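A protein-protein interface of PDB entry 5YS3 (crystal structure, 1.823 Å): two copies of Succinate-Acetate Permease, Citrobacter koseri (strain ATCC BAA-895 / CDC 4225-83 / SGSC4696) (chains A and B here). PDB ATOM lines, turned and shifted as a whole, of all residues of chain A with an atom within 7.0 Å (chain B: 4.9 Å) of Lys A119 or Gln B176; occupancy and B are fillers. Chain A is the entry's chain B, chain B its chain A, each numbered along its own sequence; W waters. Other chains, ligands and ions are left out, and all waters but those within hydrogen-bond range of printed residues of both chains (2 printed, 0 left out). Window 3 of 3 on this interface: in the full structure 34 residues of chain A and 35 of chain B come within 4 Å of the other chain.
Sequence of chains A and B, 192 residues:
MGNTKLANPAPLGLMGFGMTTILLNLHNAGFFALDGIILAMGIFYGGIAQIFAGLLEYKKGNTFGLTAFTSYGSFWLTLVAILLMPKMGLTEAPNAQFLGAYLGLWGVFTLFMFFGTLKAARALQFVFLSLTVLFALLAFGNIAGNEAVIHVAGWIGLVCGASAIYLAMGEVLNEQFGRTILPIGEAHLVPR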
ATOM      1  N   ASN A  62     -22.594  -8.006 -35.375  1.00  0.00           N
ATOM      2  CA  ASN A  62     -22.394  -7.854 -33.932  1.00  0.00           C
ATOM      3  C   ASN A  62     -23.293  -6.756 -33.370  1.00  0.00           C
ATOM      4  O   ASN A  62     -22.920  -5.590 -33.295  1.00  0.00           O
ATOM      5  CB  ASN A  62     -20.913  -7.567 -33.620  1.00  0.00           C
ATOM      6  CG  ASN A  62     -20.625  -7.461 -32.112  1.00  0.00           C
ATOM      7  OD1 ASN A  62     -21.531  -7.419 -31.294  1.00  0.00           O
ATOM      8  ND2 ASN A  62     -19.348  -7.406 -31.757  1.00  0.00           N
ATOM      9  N   THR A  63     -24.499  -7.140 -32.981  1.00  0.00           N
ATOM     10  CA  THR A  63     -25.455  -6.183 -32.441  1.00  0.00           C
ATOM     11  C   THR A  63     -24.961  -5.449 -31.190  1.00  0.00           C
ATOM     12  O   THR A  63     -25.186  -4.252 -31.038  1.00  0.00           O
ATOM     13  CB  THR A  63     -26.782  -6.900 -32.098  1.00  0.00           C
ATOM     14  OG1 THR A  63     -27.317  -7.468 -33.298  1.00  0.00           O
ATOM     15  CG2 THR A  63     -27.781  -5.932 -31.466  1.00  0.00           C
ATOM     16  N   PHE A  64     -24.326  -6.175 -30.279  1.00  0.00           N
ATOM     17  CA  PHE A  64     -23.863  -5.564 -29.035  1.00  0.00           C
ATOM     18  C   PHE A  64     -22.903  -4.437 -29.372  1.00  0.00           C
ATOM     19  O   PHE A  64     -23.037  -3.327 -28.869  1.00  0.00           O
ATOM     20  CB  PHE A  64     -23.176  -6.589 -28.127  1.00  0.00           C
ATOM     21  CG  PHE A  64     -22.753  -6.029 -26.784  1.00  0.00           C
ATOM     22  CD1 PHE A  64     -21.506  -5.427 -26.617  1.00  0.00           C
ATOM     23  CD2 PHE A  64     -23.606  -6.098 -25.699  1.00  0.00           C
ATOM     24  CE1 PHE A  64     -21.124  -4.914 -25.385  1.00  0.00           C
ATOM     25  CE2 PHE A  64     -23.229  -5.586 -24.463  1.00  0.00           C
ATOM     26  CZ  PHE A  64     -21.996  -4.993 -24.307  1.00  0.00           C
ATOM     27  N   GLY A  65     -21.948  -4.733 -30.251  1.00  0.00           N
ATOM     28  CA  GLY A  65     -20.922  -3.755 -30.610  1.00  0.00           C
ATOM     29  C   GLY A  65     -21.490  -2.565 -31.379  1.00  0.00           C
ATOM     30  O   GLY A  65     -21.114  -1.412 -31.131  1.00  0.00           O
ATOM     31  N   MET A 113     -26.186  -3.095 -20.448  1.00  0.00           N
ATOM     32  CA  MET A 113     -25.200  -3.623 -21.409  1.00  0.00           C
ATOM     33  C   MET A 113     -24.157  -4.475 -20.689  1.00  0.00           C
ATOM     34  O   MET A 113     -23.628  -5.428 -21.259  1.00  0.00           O
ATOM     35  CB  MET A 113     -24.508  -2.496 -22.196  1.00  0.00           C
ATOM     36  CG  MET A 113     -25.435  -1.695 -23.139  1.00  0.00           C
ATOM     37  SD  MET A 113     -26.024  -2.703 -24.514  1.00  0.00           S
ATOM     38  CE  MET A 113     -24.671  -2.534 -25.695  1.00  0.00           C
ATOM     39  N   PHE A 114     -23.855  -4.142 -19.435  1.00  0.00           N
ATOM     40  CA  PHE A 114     -22.923  -4.981 -18.685  1.00  0.00           C
ATOM     41  C   PHE A 114     -23.408  -6.442 -18.630  1.00  0.00           C
ATOM     42  O   PHE A 114     -22.616  -7.369 -18.774  1.00  0.00           O
ATOM     43  CB  PHE A 114     -22.707  -4.447 -17.260  1.00  0.00           C
ATOM     44  CG  PHE A 114     -22.114  -5.478 -16.336  1.00  0.00           C
ATOM     45  CD1 PHE A 114     -20.772  -5.814 -16.424  1.00  0.00           C
ATOM     46  CD2 PHE A 114     -22.908  -6.142 -15.414  1.00  0.00           C
ATOM     47  CE1 PHE A 114     -20.217  -6.774 -15.586  1.00  0.00           C
ATOM     48  CE2 PHE A 114     -22.370  -7.109 -14.583  1.00  0.00           C
ATOM     49  CZ  PHE A 114     -21.018  -7.428 -14.664  1.00  0.00           C
ATOM     50  N   PHE A 115     -24.710  -6.654 -18.442  1.00  0.00           N
ATOM     51  CA  PHE A 115     -25.227  -8.017 -18.381  1.00  0.00           C
ATOM     52  C   PHE A 115     -25.088  -8.688 -19.735  1.00  0.00           C
ATOM     53  O   PHE A 115     -24.911  -9.904 -19.816  1.00  0.00           O
ATOM     54  CB  PHE A 115     -26.680  -8.029 -17.874  1.00  0.00           C
ATOM     55  CG  PHE A 115     -26.780  -7.697 -16.411  1.00  0.00           C
ATOM     56  CD1 PHE A 115     -26.523  -8.660 -15.453  1.00  0.00           C
ATOM     57  CD2 PHE A 115     -27.071  -6.412 -15.996  1.00  0.00           C
ATOM     58  CE1 PHE A 115     -26.576  -8.348 -14.112  1.00  0.00           C
ATOM     59  CE2 PHE A 115     -27.119  -6.091 -14.659  1.00  0.00           C
ATOM     60  CZ  PHE A 115     -26.872  -7.061 -13.713  1.00  0.00           C
ATOM     61  N   GLY A 116     -25.106  -7.883 -20.796  1.00  0.00           N
ATOM     62  CA  GLY A 116     -24.729  -8.366 -22.109  1.00  0.00           C
ATOM     63  C   GLY A 116     -23.298  -8.865 -22.241  1.00  0.00           C
ATOM     64  O   GLY A 116     -23.026  -9.706 -23.098  1.00  0.00           O
ATOM     65  N   THR A 117     -22.371  -8.361 -21.426  1.00  0.00           N
ATOM     66  CA  THR A 117     -20.970  -8.769 -21.588  1.00  0.00           C
ATOM     67  C   THR A 117     -20.664 -10.083 -20.884  1.00  0.00           C
ATOM     68  O   THR A 117     -19.573 -10.635 -21.039  1.00  0.00           O
ATOM     69  CB  THR A 117     -19.985  -7.711 -21.052  1.00  0.00           C
ATOM     70  OG1 THR A 117     -20.083  -7.635 -19.627  1.00  0.00           O
ATOM     71  CG2 THR A 117     -20.284  -6.357 -21.641  1.00  0.00           C
ATOM     72  N   LEU A 118     -21.622 -10.597 -20.119  1.00  0.00           N
ATOM     73  CA  LEU A 118     -21.362 -11.795 -19.332  1.00  0.00           C
ATOM     74  C   LEU A 118     -21.118 -12.986 -20.244  1.00  0.00           C
ATOM     75  O   LEU A 118     -20.602 -14.016 -19.819  1.00  0.00           O
ATOM     76  CB  LEU A 118     -22.518 -12.069 -18.370  1.00  0.00           C
ATOM     77  CG  LEU A 118     -22.669 -10.982 -17.305  1.00  0.00           C
ATOM     78  CD1 LEU A 118     -23.931 -11.195 -16.493  1.00  0.00           C
ATOM     79  CD2 LEU A 118     -21.456 -10.944 -16.395  1.00  0.00           C
ATOM     80  N   LYS A 119     -21.483 -12.820 -21.508  1.00  0.00           N
ATOM     81  CA  LYS A 119     -21.239 -13.819 -22.526  1.00  0.00           C
ATOM     82  C   LYS A 119     -19.920 -13.554 -23.246  1.00  0.00           C
ATOM     83  O   LYS A 119     -19.497 -14.350 -24.083  1.00  0.00           O
ATOM     84  CB  LYS A 119     -22.394 -13.832 -23.532  1.00  0.00           C
ATOM     85  CG  LYS A 119     -22.953 -15.217 -23.821  1.00  0.00           C
ATOM     86  CD  LYS A 119     -23.677 -15.773 -22.611  1.00  0.00           C
ATOM     87  CE  LYS A 119     -23.565 -17.291 -22.546  1.00  0.00           C
ATOM     88  NZ  LYS A 119     -22.255 -17.733 -21.998  1.00  0.00           N
ATOM     89  N   ALA A 120     -19.271 -12.441 -22.908  1.00  0.00           N
ATOM     90  CA  ALA A 120     -18.065 -12.015 -23.611  1.00  0.00           C
ATOM     91  C   ALA A 120     -16.825 -12.015 -22.724  1.00  0.00           C
ATOM     92  O   ALA A 120     -16.879 -12.441 -21.567  1.00  0.00           O
ATOM     93  CB  ALA A 120     -18.273 -10.627 -24.213  1.00  0.00           C
ATOM     94  N   ALA A 121     -15.719 -11.513 -23.281  1.00  0.00           N
ATOM     95  CA  ALA A 121     -14.418 -11.475 -22.601  1.00  0.00           C
ATOM     96  C   ALA A 121     -14.489 -10.866 -21.203  1.00  0.00           C
ATOM     97  O   ALA A 121     -15.120  -9.831 -21.003  1.00  0.00           O
ATOM     98  CB  ALA A 121     -13.418 -10.700 -23.449  1.00  0.00           C
ATOM     99  N   LEU A 124     -13.748  -7.244 -20.991  1.00  0.00           N
ATOM    100  CA  LEU A 124     -14.840  -6.389 -21.437  1.00  0.00           C
ATOM    101  C   LEU A 124     -15.862  -6.214 -20.307  1.00  0.00           C
ATOM    102  O   LEU A 124     -16.447  -5.146 -20.133  1.00  0.00           O
ATOM    103  CB  LEU A 124     -15.509  -6.972 -22.699  1.00  0.00           C
ATOM    104  CG  LEU A 124     -16.592  -6.085 -23.334  1.00  0.00           C
ATOM    105  CD1 LEU A 124     -15.979  -4.848 -24.008  1.00  0.00           C
ATOM    106  CD2 LEU A 124     -17.470  -6.855 -24.334  1.00  0.00           C
ATOM    107  N   GLN A 125     -16.072  -7.272 -19.532  1.00  0.00           N
ATOM    108  CA  GLN A 125     -16.960  -7.190 -18.370  1.00  0.00           C
ATOM    109  C   GLN A 125     -16.455  -6.148 -17.394  1.00  0.00           C
ATOM    110  O   GLN A 125     -17.239  -5.360 -16.872  1.00  0.00           O
ATOM    111  CB  GLN A 125     -17.072  -8.550 -17.677  1.00  0.00           C
ATOM    112  CG  GLN A 125     -17.637  -9.621 -18.546  1.00  0.00           C
ATOM    113  CD  GLN A 125     -17.619 -10.979 -17.870  1.00  0.00           C
ATOM    114  OE1 GLN A 125     -17.529 -11.068 -16.647  1.00  0.00           O
ATOM    115  NE2 GLN A 125     -17.701 -12.041 -18.662  1.00  0.00           N
ATOM    116  N   VAL B 172     -31.206  -6.584 -27.180  1.00  0.00           N
ATOM    117  CA  VAL B 172     -29.771  -6.865 -27.070  1.00  0.00           C
ATOM    118  C   VAL B 172     -29.497  -8.100 -26.207  1.00  0.00           C
ATOM    119  O   VAL B 172     -28.795  -9.019 -26.649  1.00  0.00           O
ATOM    120  CB  VAL B 172     -28.980  -5.676 -26.482  1.00  0.00           C
ATOM    121  CG1 VAL B 172     -27.549  -6.095 -26.181  1.00  0.00           C
ATOM    122  CG2 VAL B 172     -28.999  -4.500 -27.444  1.00  0.00           C
ATOM    123  N   LEU B 173     -30.054  -8.128 -24.991  1.00  0.00           N
ATOM    124  CA  LEU B 173     -29.783  -9.241 -24.070  1.00  0.00           C
ATOM    125  C   LEU B 173     -30.337 -10.560 -24.589  1.00  0.00           C
ATOM    126  O   LEU B 173     -29.672 -11.597 -24.501  1.00  0.00           O
ATOM    127  CB  LEU B 173     -30.353  -8.954 -22.671  1.00  0.00           C
ATOM    128  CG  LEU B 173     -29.698  -7.757 -21.990  1.00  0.00           C
ATOM    129  CD1 LEU B 173     -30.178  -7.577 -20.561  1.00  0.00           C
ATOM    130  CD2 LEU B 173     -28.189  -7.929 -22.042  1.00  0.00           C
ATOM    131  N   ASN B 174     -31.545 -10.523 -25.134  1.00  0.00           N
ATOM    132  CA  ASN B 174     -32.157 -11.734 -25.645  1.00  0.00           C
ATOM    133  C   ASN B 174     -31.335 -12.316 -26.782  1.00  0.00           C
ATOM    134  O   ASN B 174     -31.195 -13.529 -26.881  1.00  0.00           O
ATOM    135  CB  ASN B 174     -33.598 -11.487 -26.108  1.00  0.00           C
ATOM    136  CG  ASN B 174     -34.541 -11.167 -24.955  1.00  0.00           C
ATOM    137  OD1 ASN B 174     -34.160 -11.237 -23.784  1.00  0.00           O
ATOM    138  ND2 ASN B 174     -35.782 -10.822 -25.283  1.00  0.00           N
ATOM    139  N   GLU B 175     -30.752 -11.453 -27.616  1.00  0.00           N
ATOM    140  CA  GLU B 175     -29.863 -11.937 -28.674  1.00  0.00           C
ATOM    141  C   GLU B 175     -28.545 -12.434 -28.089  1.00  0.00           C
ATOM    142  O   GLU B 175     -28.068 -13.489 -28.488  1.00  0.00           O
ATOM    143  CB  GLU B 175     -29.602 -10.859 -29.750  1.00  0.00           C
ATOM    144  CG  GLU B 175     -28.652 -11.347 -30.869  1.00  0.00           C
ATOM    145  CD  GLU B 175     -28.431 -10.352 -32.026  1.00  0.00           C
ATOM    146  OE1 GLU B 175     -27.513 -10.589 -32.841  1.00  0.00           O
ATOM    147  OE2 GLU B 175     -29.167  -9.357 -32.146  1.00  0.00           O
ATOM    148  N   GLN B 176     -27.960 -11.691 -27.145  1.00  0.00           N
ATOM    149  CA  GLN B 176     -26.680 -12.096 -26.557  1.00  0.00           C
ATOM    150  C   GLN B 176     -26.769 -13.481 -25.918  1.00  0.00           C
ATOM    151  O   GLN B 176     -25.870 -14.295 -26.081  1.00  0.00           O
ATOM    152  CB  GLN B 176     -26.205 -11.099 -25.495  1.00  0.00           C
ATOM    153  CG  GLN B 176     -25.628  -9.804 -26.023  1.00  0.00           C
ATOM    154  CD  GLN B 176     -24.348 -10.005 -26.836  1.00  0.00           C
ATOM    155  OE1 GLN B 176     -24.397 -10.306 -28.024  1.00  0.00           O
ATOM    156  NE2 GLN B 176     -23.200  -9.825 -26.194  1.00  0.00           N
ATOM    157  N   PHE B 177     -27.850 -13.745 -25.190  1.00  0.00           N
ATOM    158  CA  PHE B 177     -27.986 -15.030 -24.496  1.00  0.00           C
ATOM    159  C   PHE B 177     -28.686 -16.120 -25.317  1.00  0.00           C
ATOM    160  O   PHE B 177     -28.729 -17.278 -24.904  1.00  0.00           O
ATOM    161  CB  PHE B 177     -28.735 -14.840 -23.183  1.00  0.00           C
ATOM    162  CG  PHE B 177     -27.935 -14.139 -22.120  1.00  0.00           C
ATOM    163  CD1 PHE B 177     -27.839 -12.759 -22.101  1.00  0.00           C
ATOM    164  CD2 PHE B 177     -27.290 -14.865 -21.128  1.00  0.00           C
ATOM    165  CE1 PHE B 177     -27.110 -12.109 -21.118  1.00  0.00           C
ATOM    166  CE2 PHE B 177     -26.558 -14.223 -20.138  1.00  0.00           C
ATOM    167  CZ  PHE B 177     -26.466 -12.844 -20.134  1.00  0.00           C
ATOM    168  N   GLY B 178     -29.240 -15.758 -26.468  1.00  0.00           N
ATOM    169  CA  GLY B 178     -29.885 -16.737 -27.334  1.00  0.00           C
ATOM    170  C   GLY B 178     -31.190 -17.276 -26.764  1.00  0.00           C
ATOM    171  O   GLY B 178     -31.614 -18.367 -27.107  1.00  0.00           O
HETATM  172  O   HOH W   1     -25.009 -10.098 -32.469  1.00  0.00           O
HETATM  173  O   HOH W   2     -24.027  -9.182 -30.359  1.00  0.00           O
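O of Gly A116 lies within hydrogen-bond range of NE2 of Gln B176 (3.1 Å).
The side-chain carboxylate of Glu B175 sits at hydrogen-bond distance from the side-chain hydroxyl of Thr A63, 2.9 Å away.
The backbone NH (N) of Phe A64 sits at hydrogen-bond distance from the side-chain amide oxygen (OD1) of Asn A62, at 3.2 Å.
Phe A64 touches Val B172.
Phe A64 touches Gln B176 (CB to NE2, 3.8 Å).
Phe A115 touches Leu B173 (C to CD2, 3.9 Å).
CZ of Phe B177 touches O of Phe A115, at 3.3 Å.
N of Gly A116 touches CD2 of Leu B173, at 3.3 Å.
O of Gln B176 touches CG of Lys A119 (3.8 Å).
Of the printed residues of chain B, Lys A119 touches Gln B176.
Printed residues of chain A within 4 Å of Phe B177: Phe A115.
Printed residues of chain B within 4 Å of Phe A64: Val B172 and Gln B176.
Of the printed residues of chain B, Thr A63 touches Glu B175.
Printed residues of chain B within 4 Å of Phe A115: Leu B173 (3.9 Å) and Phe B177 (3.3 Å).
Printed residues of chain A within 4 Å of Leu B173: Phe A115 and Gly A116.
The nearest printed residue of chain B that does not touch Lys A119 is Phe B177 (4.01 Å).
Of the 7 printed residues of chain B, 5 touch a printed residue of chain A.
Of the 15 printed residues of chain A, 5 touch a printed residue of chain B.
Hydrophobic or aromatic side chains of chain A that line the printed part of chain B: Phe A64.
Among the printed residues, no Asp or Glu carboxylate lies within 4 Å of a Lys or Arg side-chain nitrogen of the other chain.
No position is printed for both chains.
Of the 8 pairs that touch across the chains among the printed residues, none has its exchanged pair printed and touching as well.
Water W1 lies within hydrogen-bond range of the side-chain carboxylate (OE1) of Glu B175 (2.6 Å) and the backbone NH (N) of Thr A63 (3.0 Å).
Water W2 lies within hydrogen-bond range of the side-chain amide oxygen of Gln B176, the backbone NH of Phe A64, the side-chain amide oxygen of Asn A62 and the backbone NH of Thr A63.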
